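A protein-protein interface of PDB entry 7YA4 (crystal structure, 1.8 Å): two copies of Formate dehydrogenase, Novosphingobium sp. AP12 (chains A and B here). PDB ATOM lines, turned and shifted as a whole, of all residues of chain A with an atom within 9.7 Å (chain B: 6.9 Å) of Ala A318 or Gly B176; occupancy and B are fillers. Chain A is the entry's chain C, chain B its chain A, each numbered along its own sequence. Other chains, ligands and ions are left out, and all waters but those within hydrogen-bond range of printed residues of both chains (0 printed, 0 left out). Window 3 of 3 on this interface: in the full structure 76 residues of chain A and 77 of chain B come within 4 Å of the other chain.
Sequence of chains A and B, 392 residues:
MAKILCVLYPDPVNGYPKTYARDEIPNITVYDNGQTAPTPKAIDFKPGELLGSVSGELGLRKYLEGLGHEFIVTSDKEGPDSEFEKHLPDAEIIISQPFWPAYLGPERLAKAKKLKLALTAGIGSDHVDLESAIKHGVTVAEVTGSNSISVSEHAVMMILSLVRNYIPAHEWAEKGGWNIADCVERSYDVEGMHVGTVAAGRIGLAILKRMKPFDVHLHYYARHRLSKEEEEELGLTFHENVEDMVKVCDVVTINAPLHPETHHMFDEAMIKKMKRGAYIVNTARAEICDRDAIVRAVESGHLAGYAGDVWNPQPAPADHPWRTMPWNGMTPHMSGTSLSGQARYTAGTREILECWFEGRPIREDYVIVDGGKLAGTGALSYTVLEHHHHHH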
ATOM      1  N   TRP A 311      -4.475  26.985 -23.789  1.00  0.00           N
ATOM      2  CA  TRP A 311      -4.670  26.307 -22.517  1.00  0.00           C
ATOM      3  C   TRP A 311      -3.603  25.245 -22.322  1.00  0.00           C
ATOM      4  O   TRP A 311      -3.060  24.738 -23.302  1.00  0.00           O
ATOM      5  CB  TRP A 311      -6.038  25.606 -22.492  1.00  0.00           C
ATOM      6  CG  TRP A 311      -7.199  26.489 -22.836  1.00  0.00           C
ATOM      7  CD1 TRP A 311      -7.546  26.969 -24.074  1.00  0.00           C
ATOM      8  CD2 TRP A 311      -8.185  26.975 -21.911  1.00  0.00           C
ATOM      9  NE1 TRP A 311      -8.676  27.741 -23.980  1.00  0.00           N
ATOM     10  CE2 TRP A 311      -9.086  27.768 -22.666  1.00  0.00           C
ATOM     11  CE3 TRP A 311      -8.370  26.854 -20.519  1.00  0.00           C
ATOM     12  CZ2 TRP A 311     -10.190  28.386 -22.070  1.00  0.00           C
ATOM     13  CZ3 TRP A 311      -9.440  27.497 -19.935  1.00  0.00           C
ATOM     14  CH2 TRP A 311     -10.348  28.234 -20.703  1.00  0.00           C
ATOM     15  N   ASN A 312      -3.418  24.834 -21.055  1.00  0.00           N
ATOM     16  CA  ASN A 312      -2.621  23.659 -20.766  1.00  0.00           C
ATOM     17  C   ASN A 312      -3.395  22.789 -19.789  1.00  0.00           C
ATOM     18  O   ASN A 312      -3.694  23.244 -18.702  1.00  0.00           O
ATOM     19  CB  ASN A 312      -1.257  23.984 -20.155  1.00  0.00           C
ATOM     20  CG  ASN A 312      -0.414  22.728 -20.091  1.00  0.00           C
ATOM     21  OD1 ASN A 312      -0.240  22.052 -21.103  1.00  0.00           O
ATOM     22  ND2 ASN A 312       0.073  22.379 -18.910  1.00  0.00           N
ATOM     23  N   PRO A 313      -3.686  21.505 -20.064  1.00  0.00           N
ATOM     24  CA  PRO A 313      -3.451  20.861 -21.347  1.00  0.00           C
ATOM     25  C   PRO A 313      -4.447  21.408 -22.360  1.00  0.00           C
ATOM     26  O   PRO A 313      -5.331  22.192 -22.005  1.00  0.00           O
ATOM     27  CB  PRO A 313      -3.633  19.343 -21.091  1.00  0.00           C
ATOM     28  CG  PRO A 313      -4.399  19.267 -19.787  1.00  0.00           C
ATOM     29  CD  PRO A 313      -4.188  20.571 -19.044  1.00  0.00           C
ATOM     30  N   PRO A 315      -6.959  19.841 -25.601  1.00  0.00           N
ATOM     31  CA  PRO A 315      -8.074  20.602 -25.024  1.00  0.00           C
ATOM     32  C   PRO A 315      -8.025  20.723 -23.500  1.00  0.00           C
ATOM     33  O   PRO A 315      -7.532  19.821 -22.836  1.00  0.00           O
ATOM     34  CB  PRO A 315      -9.311  19.767 -25.382  1.00  0.00           C
ATOM     35  CG  PRO A 315      -8.923  19.023 -26.652  1.00  0.00           C
ATOM     36  CD  PRO A 315      -7.440  18.754 -26.485  1.00  0.00           C
ATOM     37  N   ALA A 316      -8.586  21.804 -22.962  1.00  0.00           N
ATOM     38  CA  ALA A 316      -8.578  22.030 -21.528  1.00  0.00           C
ATOM     39  C   ALA A 316      -9.568  21.059 -20.905  1.00  0.00           C
ATOM     40  O   ALA A 316     -10.680  20.927 -21.399  1.00  0.00           O
ATOM     41  CB  ALA A 316      -8.942  23.459 -21.209  1.00  0.00           C
ATOM     42  N   PRO A 317      -9.230  20.406 -19.779  1.00  0.00           N
ATOM     43  CA  PRO A 317     -10.224  19.662 -19.015  1.00  0.00           C
ATOM     44  C   PRO A 317     -11.397  20.563 -18.605  1.00  0.00           C
ATOM     45  O   PRO A 317     -11.238  21.787 -18.450  1.00  0.00           O
ATOM     46  CB  PRO A 317      -9.439  19.180 -17.780  1.00  0.00           C
ATOM     47  CG  PRO A 317      -7.996  19.210 -18.207  1.00  0.00           C
ATOM     48  CD  PRO A 317      -7.907  20.415 -19.123  1.00  0.00           C
ATOM     49  N   ALA A 318     -12.564  19.949 -18.383  1.00  0.00           N
ATOM     50  CA  ALA A 318     -13.784  20.680 -18.061  1.00  0.00           C
ATOM     51  C   ALA A 318     -13.645  21.513 -16.777  1.00  0.00           C
ATOM     52  O   ALA A 318     -14.313  22.536 -16.672  1.00  0.00           O
ATOM     53  CB  ALA A 318     -14.976  19.723 -18.005  1.00  0.00           C
ATOM     54  N   ASP A 319     -12.770  21.114 -15.840  1.00  0.00           N
ATOM     55  CA  ASP A 319     -12.568  21.818 -14.576  1.00  0.00           C
ATOM     56  C   ASP A 319     -11.334  22.722 -14.561  1.00  0.00           C
ATOM     57  O   ASP A 319     -10.927  23.181 -13.489  1.00  0.00           O
ATOM     58  CB  ASP A 319     -12.375  20.835 -13.411  1.00  0.00           C
ATOM     59  CG  ASP A 319     -11.164  19.908 -13.532  1.00  0.00           C
ATOM     60  OD1 ASP A 319     -10.432  19.941 -14.580  1.00  0.00           O
ATOM     61  OD2 ASP A 319     -10.957  19.127 -12.592  1.00  0.00           O
ATOM     62  N   HIS A 320     -10.724  22.970 -15.717  1.00  0.00           N
ATOM     63  CA  HIS A 320      -9.556  23.847 -15.778  1.00  0.00           C
ATOM     64  C   HIS A 320      -9.870  25.174 -15.096  1.00  0.00           C
ATOM     65  O   HIS A 320     -10.903  25.784 -15.367  1.00  0.00           O
ATOM     66  CB  HIS A 320      -9.139  24.055 -17.250  1.00  0.00           C
ATOM     67  CG  HIS A 320      -7.810  24.721 -17.423  1.00  0.00           C
ATOM     68  ND1 HIS A 320      -7.579  26.040 -17.107  1.00  0.00           N
ATOM     69  CD2 HIS A 320      -6.616  24.198 -17.837  1.00  0.00           C
ATOM     70  CE1 HIS A 320      -6.295  26.322 -17.339  1.00  0.00           C
ATOM     71  NE2 HIS A 320      -5.669  25.199 -17.804  1.00  0.00           N
ATOM     72  N   PRO A 321      -9.028  25.653 -14.152  1.00  0.00           N
ATOM     73  CA  PRO A 321      -9.382  26.824 -13.352  1.00  0.00           C
ATOM     74  C   PRO A 321      -9.440  28.149 -14.119  1.00  0.00           C
ATOM     75  O   PRO A 321     -10.109  29.055 -13.661  1.00  0.00           O
ATOM     76  CB  PRO A 321      -8.304  26.875 -12.264  1.00  0.00           C
ATOM     77  CG  PRO A 321      -7.115  26.174 -12.902  1.00  0.00           C
ATOM     78  CD  PRO A 321      -7.748  25.058 -13.726  1.00  0.00           C
ATOM     79  N   TRP A 322      -8.819  28.235 -15.300  1.00  0.00           N
ATOM     80  CA  TRP A 322      -8.912  29.463 -16.104  1.00  0.00           C
ATOM     81  C   TRP A 322     -10.333  29.696 -16.629  1.00  0.00           C
ATOM     82  O   TRP A 322     -10.721  30.829 -16.942  1.00  0.00           O
ATOM     83  CB  TRP A 322      -7.924  29.445 -17.259  1.00  0.00           C
ATOM     84  CG  TRP A 322      -6.517  29.698 -16.846  1.00  0.00           C
ATOM     85  CD1 TRP A 322      -6.044  29.857 -15.580  1.00  0.00           C
ATOM     86  CD2 TRP A 322      -5.381  29.740 -17.714  1.00  0.00           C
ATOM     87  NE1 TRP A 322      -4.700  30.068 -15.610  1.00  0.00           N
ATOM     88  CE2 TRP A 322      -4.258  29.988 -16.907  1.00  0.00           C
ATOM     89  CE3 TRP A 322      -5.199  29.632 -19.101  1.00  0.00           C
ATOM     90  CZ2 TRP A 322      -2.968  30.092 -17.431  1.00  0.00           C
ATOM     91  CZ3 TRP A 322      -3.919  29.738 -19.608  1.00  0.00           C
ATOM     92  CH2 TRP A 322      -2.827  30.024 -18.796  1.00  0.00           C
ATOM     93  N   ARG A 323     -11.145  28.628 -16.687  1.00  0.00           N
ATOM     94  CA  ARG A 323     -12.507  28.753 -17.185  1.00  0.00           C
ATOM     95  C   ARG A 323     -13.393  29.655 -16.321  1.00  0.00           C
ATOM     96  O   ARG A 323     -14.273  30.327 -16.873  1.00  0.00           O
ATOM     97  CB  ARG A 323     -13.201  27.382 -17.315  1.00  0.00           C
ATOM     98  CG  ARG A 323     -12.540  26.441 -18.304  1.00  0.00           C
ATOM     99  CD  ARG A 323     -13.126  25.041 -18.226  1.00  0.00           C
ATOM    100  NE  ARG A 323     -12.682  24.138 -19.279  1.00  0.00           N
ATOM    101  CZ  ARG A 323     -13.187  24.038 -20.506  1.00  0.00           C
ATOM    102  NH1 ARG A 323     -14.128  24.857 -20.958  1.00  0.00           N
ATOM    103  NH2 ARG A 323     -12.771  23.048 -21.270  1.00  0.00           N
ATOM    104  N   THR A 324     -13.194  29.636 -14.985  1.00  0.00           N
ATOM    105  CA  THR A 324     -14.145  30.208 -14.050  1.00  0.00           C
ATOM    106  C   THR A 324     -13.463  31.200 -13.101  1.00  0.00           C
ATOM    107  O   THR A 324     -14.122  31.717 -12.199  1.00  0.00           O
ATOM    108  CB  THR A 324     -14.851  29.097 -13.243  1.00  0.00           C
ATOM    109  OG1 THR A 324     -13.884  28.255 -12.610  1.00  0.00           O
ATOM    110  CG2 THR A 324     -15.753  28.231 -14.104  1.00  0.00           C
ATOM    111  N   MET A 330     -11.556  34.185 -21.468  1.00  0.00           N
ATOM    112  CA  MET A 330     -11.098  33.017 -22.219  1.00  0.00           C
ATOM    113  C   MET A 330     -12.072  32.620 -23.336  1.00  0.00           C
ATOM    114  O   MET A 330     -13.263  32.897 -23.287  1.00  0.00           O
ATOM    115  CB  MET A 330     -10.953  31.775 -21.320  1.00  0.00           C
ATOM    116  CG  MET A 330      -9.970  31.887 -20.162  1.00  0.00           C
ATOM    117  SD  MET A 330      -8.289  32.358 -20.568  1.00  0.00           S
ATOM    118  CE  MET A 330      -7.784  30.920 -21.519  1.00  0.00           C
ATOM    119  N   PRO A 332     -12.221  28.837 -26.049  1.00  0.00           N
ATOM    120  CA  PRO A 332     -11.501  27.666 -26.555  1.00  0.00           C
ATOM    121  C   PRO A 332     -10.579  28.076 -27.686  1.00  0.00           C
ATOM    122  O   PRO A 332     -10.627  29.205 -28.192  1.00  0.00           O
ATOM    123  CB  PRO A 332     -12.623  26.723 -27.027  1.00  0.00           C
ATOM    124  CG  PRO A 332     -13.855  27.219 -26.306  1.00  0.00           C
ATOM    125  CD  PRO A 332     -13.662  28.723 -26.265  1.00  0.00           C
ATOM    126  N   GLU B 171     -18.755  31.671 -23.586  1.00  0.00           N
ATOM    127  CA  GLU B 171     -19.749  30.877 -22.875  1.00  0.00           C
ATOM    128  C   GLU B 171     -19.396  29.391 -22.955  1.00  0.00           C
ATOM    129  O   GLU B 171     -19.505  28.707 -21.945  1.00  0.00           O
ATOM    130  CB  GLU B 171     -21.151  31.180 -23.382  1.00  0.00           C
ATOM    131  CG  GLU B 171     -21.657  32.565 -23.020  1.00  0.00           C
ATOM    132  CD  GLU B 171     -22.997  32.949 -23.628  1.00  0.00           C
ATOM    133  OE1 GLU B 171     -23.575  32.125 -24.376  1.00  0.00           O
ATOM    134  OE2 GLU B 171     -23.462  34.098 -23.395  1.00  0.00           O
ATOM    135  N   TRP B 172     -19.006  28.875 -24.128  1.00  0.00           N
ATOM    136  CA  TRP B 172     -18.483  27.501 -24.232  1.00  0.00           C
ATOM    137  C   TRP B 172     -17.322  27.235 -23.260  1.00  0.00           C
ATOM    138  O   TRP B 172     -17.267  26.189 -22.626  1.00  0.00           O
ATOM    139  CB  TRP B 172     -18.052  27.170 -25.663  1.00  0.00           C
ATOM    140  CG  TRP B 172     -19.178  26.915 -26.625  1.00  0.00           C
ATOM    141  CD1 TRP B 172     -19.508  27.641 -27.734  1.00  0.00           C
ATOM    142  CD2 TRP B 172     -20.101  25.813 -26.588  1.00  0.00           C
ATOM    143  NE1 TRP B 172     -20.596  27.086 -28.363  1.00  0.00           N
ATOM    144  CE2 TRP B 172     -20.953  25.939 -27.710  1.00  0.00           C
ATOM    145  CE3 TRP B 172     -20.260  24.709 -25.734  1.00  0.00           C
ATOM    146  CZ2 TRP B 172     -21.985  25.030 -27.961  1.00  0.00           C
ATOM    147  CZ3 TRP B 172     -21.293  23.821 -25.976  1.00  0.00           C
ATOM    148  CH2 TRP B 172     -22.136  23.984 -27.082  1.00  0.00           C
ATOM    149  N   ALA B 173     -16.338  28.150 -23.177  1.00  0.00           N
ATOM    150  CA  ALA B 173     -15.214  27.987 -22.253  1.00  0.00           C
ATOM    151  C   ALA B 173     -15.666  27.995 -20.793  1.00  0.00           C
ATOM    152  O   ALA B 173     -15.224  27.149 -20.001  1.00  0.00           O
ATOM    153  CB  ALA B 173     -14.190  29.082 -22.452  1.00  0.00           C
ATOM    154  N   GLU B 174     -16.508  28.982 -20.420  1.00  0.00           N
ATOM    155  CA  GLU B 174     -16.907  29.163 -19.026  1.00  0.00           C
ATOM    156  C   GLU B 174     -17.685  27.946 -18.501  1.00  0.00           C
ATOM    157  O   GLU B 174     -17.579  27.609 -17.313  1.00  0.00           O
ATOM    158  CB  GLU B 174     -17.763  30.434 -18.866  1.00  0.00           C
ATOM    159  CG  GLU B 174     -18.040  30.815 -17.421  1.00  0.00           C
ATOM    160  CD  GLU B 174     -19.254  30.140 -16.788  1.00  0.00           C
ATOM    161  OE1 GLU B 174     -20.167  29.656 -17.518  1.00  0.00           O
ATOM    162  OE2 GLU B 174     -19.252  29.996 -15.574  1.00  0.00           O
ATOM    163  N   LYS B 175     -18.458  27.327 -19.390  1.00  0.00           N
ATOM    164  CA  LYS B 175     -19.371  26.234 -19.023  1.00  0.00           C
ATOM    165  C   LYS B 175     -18.676  24.876 -19.028  1.00  0.00           C
ATOM    166  O   LYS B 175     -19.312  23.867 -18.713  1.00  0.00           O
ATOM    167  CB  LYS B 175     -20.559  26.235 -19.998  1.00  0.00           C
ATOM    168  CG  LYS B 175     -21.569  27.340 -19.696  1.00  0.00           C
ATOM    169  CD  LYS B 175     -22.609  27.650 -20.758  1.00  0.00           C
ATOM    170  CE  LYS B 175     -23.588  28.683 -20.240  1.00  0.00           C
ATOM    171  NZ  LYS B 175     -24.292  29.373 -21.334  1.00  0.00           N
ATOM    172  N   GLY B 176     -17.401  24.811 -19.418  1.00  0.00           N
ATOM    173  CA  GLY B 176     -16.653  23.556 -19.407  1.00  0.00           C
ATOM    174  C   GLY B 176     -16.583  22.841 -20.762  1.00  0.00           C
ATOM    175  O   GLY B 176     -16.097  21.714 -20.826  1.00  0.00           O
ATOM    176  N   GLY B 177     -16.979  23.519 -21.847  1.00  0.00           N
ATOM    177  CA  GLY B 177     -16.975  22.919 -23.178  1.00  0.00           C
ATOM    178  C   GLY B 177     -15.653  23.137 -23.919  1.00  0.00           C
ATOM    179  O   GLY B 177     -14.677  23.627 -23.371  1.00  0.00           O
ATOM    180  N   TRP B 178     -15.645  22.853 -25.220  1.00  0.00           N
ATOM    181  CA  TRP B 178     -14.478  23.071 -26.055  1.00  0.00           C
ATOM    182  C   TRP B 178     -14.986  23.491 -27.439  1.00  0.00           C
ATOM    183  O   TRP B 178     -14.973  24.680 -27.796  1.00  0.00           O
ATOM    184  CB  TRP B 178     -13.551  21.832 -26.035  1.00  0.00           C
ATOM    185  CG  TRP B 178     -12.209  22.063 -26.665  1.00  0.00           C
ATOM    186  CD1 TRP B 178     -11.740  21.479 -27.798  1.00  0.00           C
ATOM    187  CD2 TRP B 178     -11.156  22.949 -26.203  1.00  0.00           C
ATOM    188  NE1 TRP B 178     -10.488  21.929 -28.085  1.00  0.00           N
ATOM    189  CE2 TRP B 178     -10.110  22.853 -27.142  1.00  0.00           C
ATOM    190  CE3 TRP B 178     -10.995  23.785 -25.087  1.00  0.00           C
ATOM    191  CZ2 TRP B 178      -8.923  23.567 -27.005  1.00  0.00           C
ATOM    192  CZ3 TRP B 178      -9.846  24.532 -24.978  1.00  0.00           C
ATOM    193  CH2 TRP B 178      -8.812  24.402 -25.911  1.00  0.00           C
ATOM    194  N   ASN B 179     -15.581  22.527 -28.145  1.00  0.00           N
ATOM    195  CA  ASN B 179     -16.593  22.840 -29.131  1.00  0.00           C
ATOM    196  C   ASN B 179     -16.049  23.835 -30.165  1.00  0.00           C
ATOM    197  O   ASN B 179     -16.755  24.766 -30.520  1.00  0.00           O
ATOM    198  CB  ASN B 179     -17.851  23.384 -28.441  1.00  0.00           C
ATOM    199  CG  ASN B 179     -18.521  22.337 -27.569  1.00  0.00           C
ATOM    200  OD1 ASN B 179     -18.148  22.156 -26.412  1.00  0.00           O
ATOM    201  ND2 ASN B 179     -19.503  21.647 -28.122  1.00  0.00           N
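No position is printed for both chains.
The backbone carbonyl oxygen of Trp B172 is in hydrogen-bond range of the backbone NH of Gly B177, 2.8 Å away. O of Ala A316 sits at hydrogen-bond distance from NH2 of Arg A323 (3.0 Å). O of Pro A317 lies within hydrogen-bond range of NE of Arg A323, at 2.9 Å. O of Ala A318 sits close to NE of Arg A323 (3.5 Å).
Of the printed residues of chain B, Pro A315 touches Trp B178. Ala A318 touches just one residue of chain B: Gly B176. Printed residues of chain B within 4 Å of Arg A323: Trp B172, Ala B173, Glu B174, Gly B176 and Gly B177. Printed residues of chain B within 4 Å of Pro A332: Ala B173 and Trp B178. Gly B176 touches just these residues of chain A: Ala A318 (3.6 Å) and Arg A323 (3.2 Å). Of the printed residues of chain A, Trp B178 touches Trp A311, Pro A315, Ala A316 and Pro A332. The nearest printed residue of chain A that does not touch Ala B173 is Met A330 (4.01 Å).
Among the printed residues, merely in contact across the chains: Trp A311 with Trp B178 (3.4 Å), Pro A315 with Trp B178 (3.6 Å), Ala A316 with Trp B178 (3.6 Å), Ala A318 with Gly B176 (3.6 Å), Arg A323 with Trp B172 (3.8 Å), Arg A323 with Glu B174 (3.6 Å), Arg A323 with Gly B176 (3.2 Å), Thr A324 with Glu B174 (3.7 Å), Pro A332 with Ala B173 (3.9 Å) and Pro A332 with Trp B178 (3.1 Å).
The backbone carbonyl oxygen of Ala B173 is in hydrogen-bond range of the guanidinium group of Arg A323, 2.7 Å away. The backbone carbonyl oxygen (O) of Gly B177 is in hydrogen-bond range of the guanidinium group (NH1) of Arg A323, 2.8 Å away.
Of the 9 printed residues of chain B, 6 touch a printed residue of chain A. Hydrophobic or aromatic side chains of chain B that line the printed part of chain A: Ala B173 and Trp B178. Hydrophobic or aromatic side chains of chain A within 4 Å of the printed part of chain B: Trp A311, Pro A315, Ala A318 and Pro A332. Among the printed residues, 12 pairs touch across the chains.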
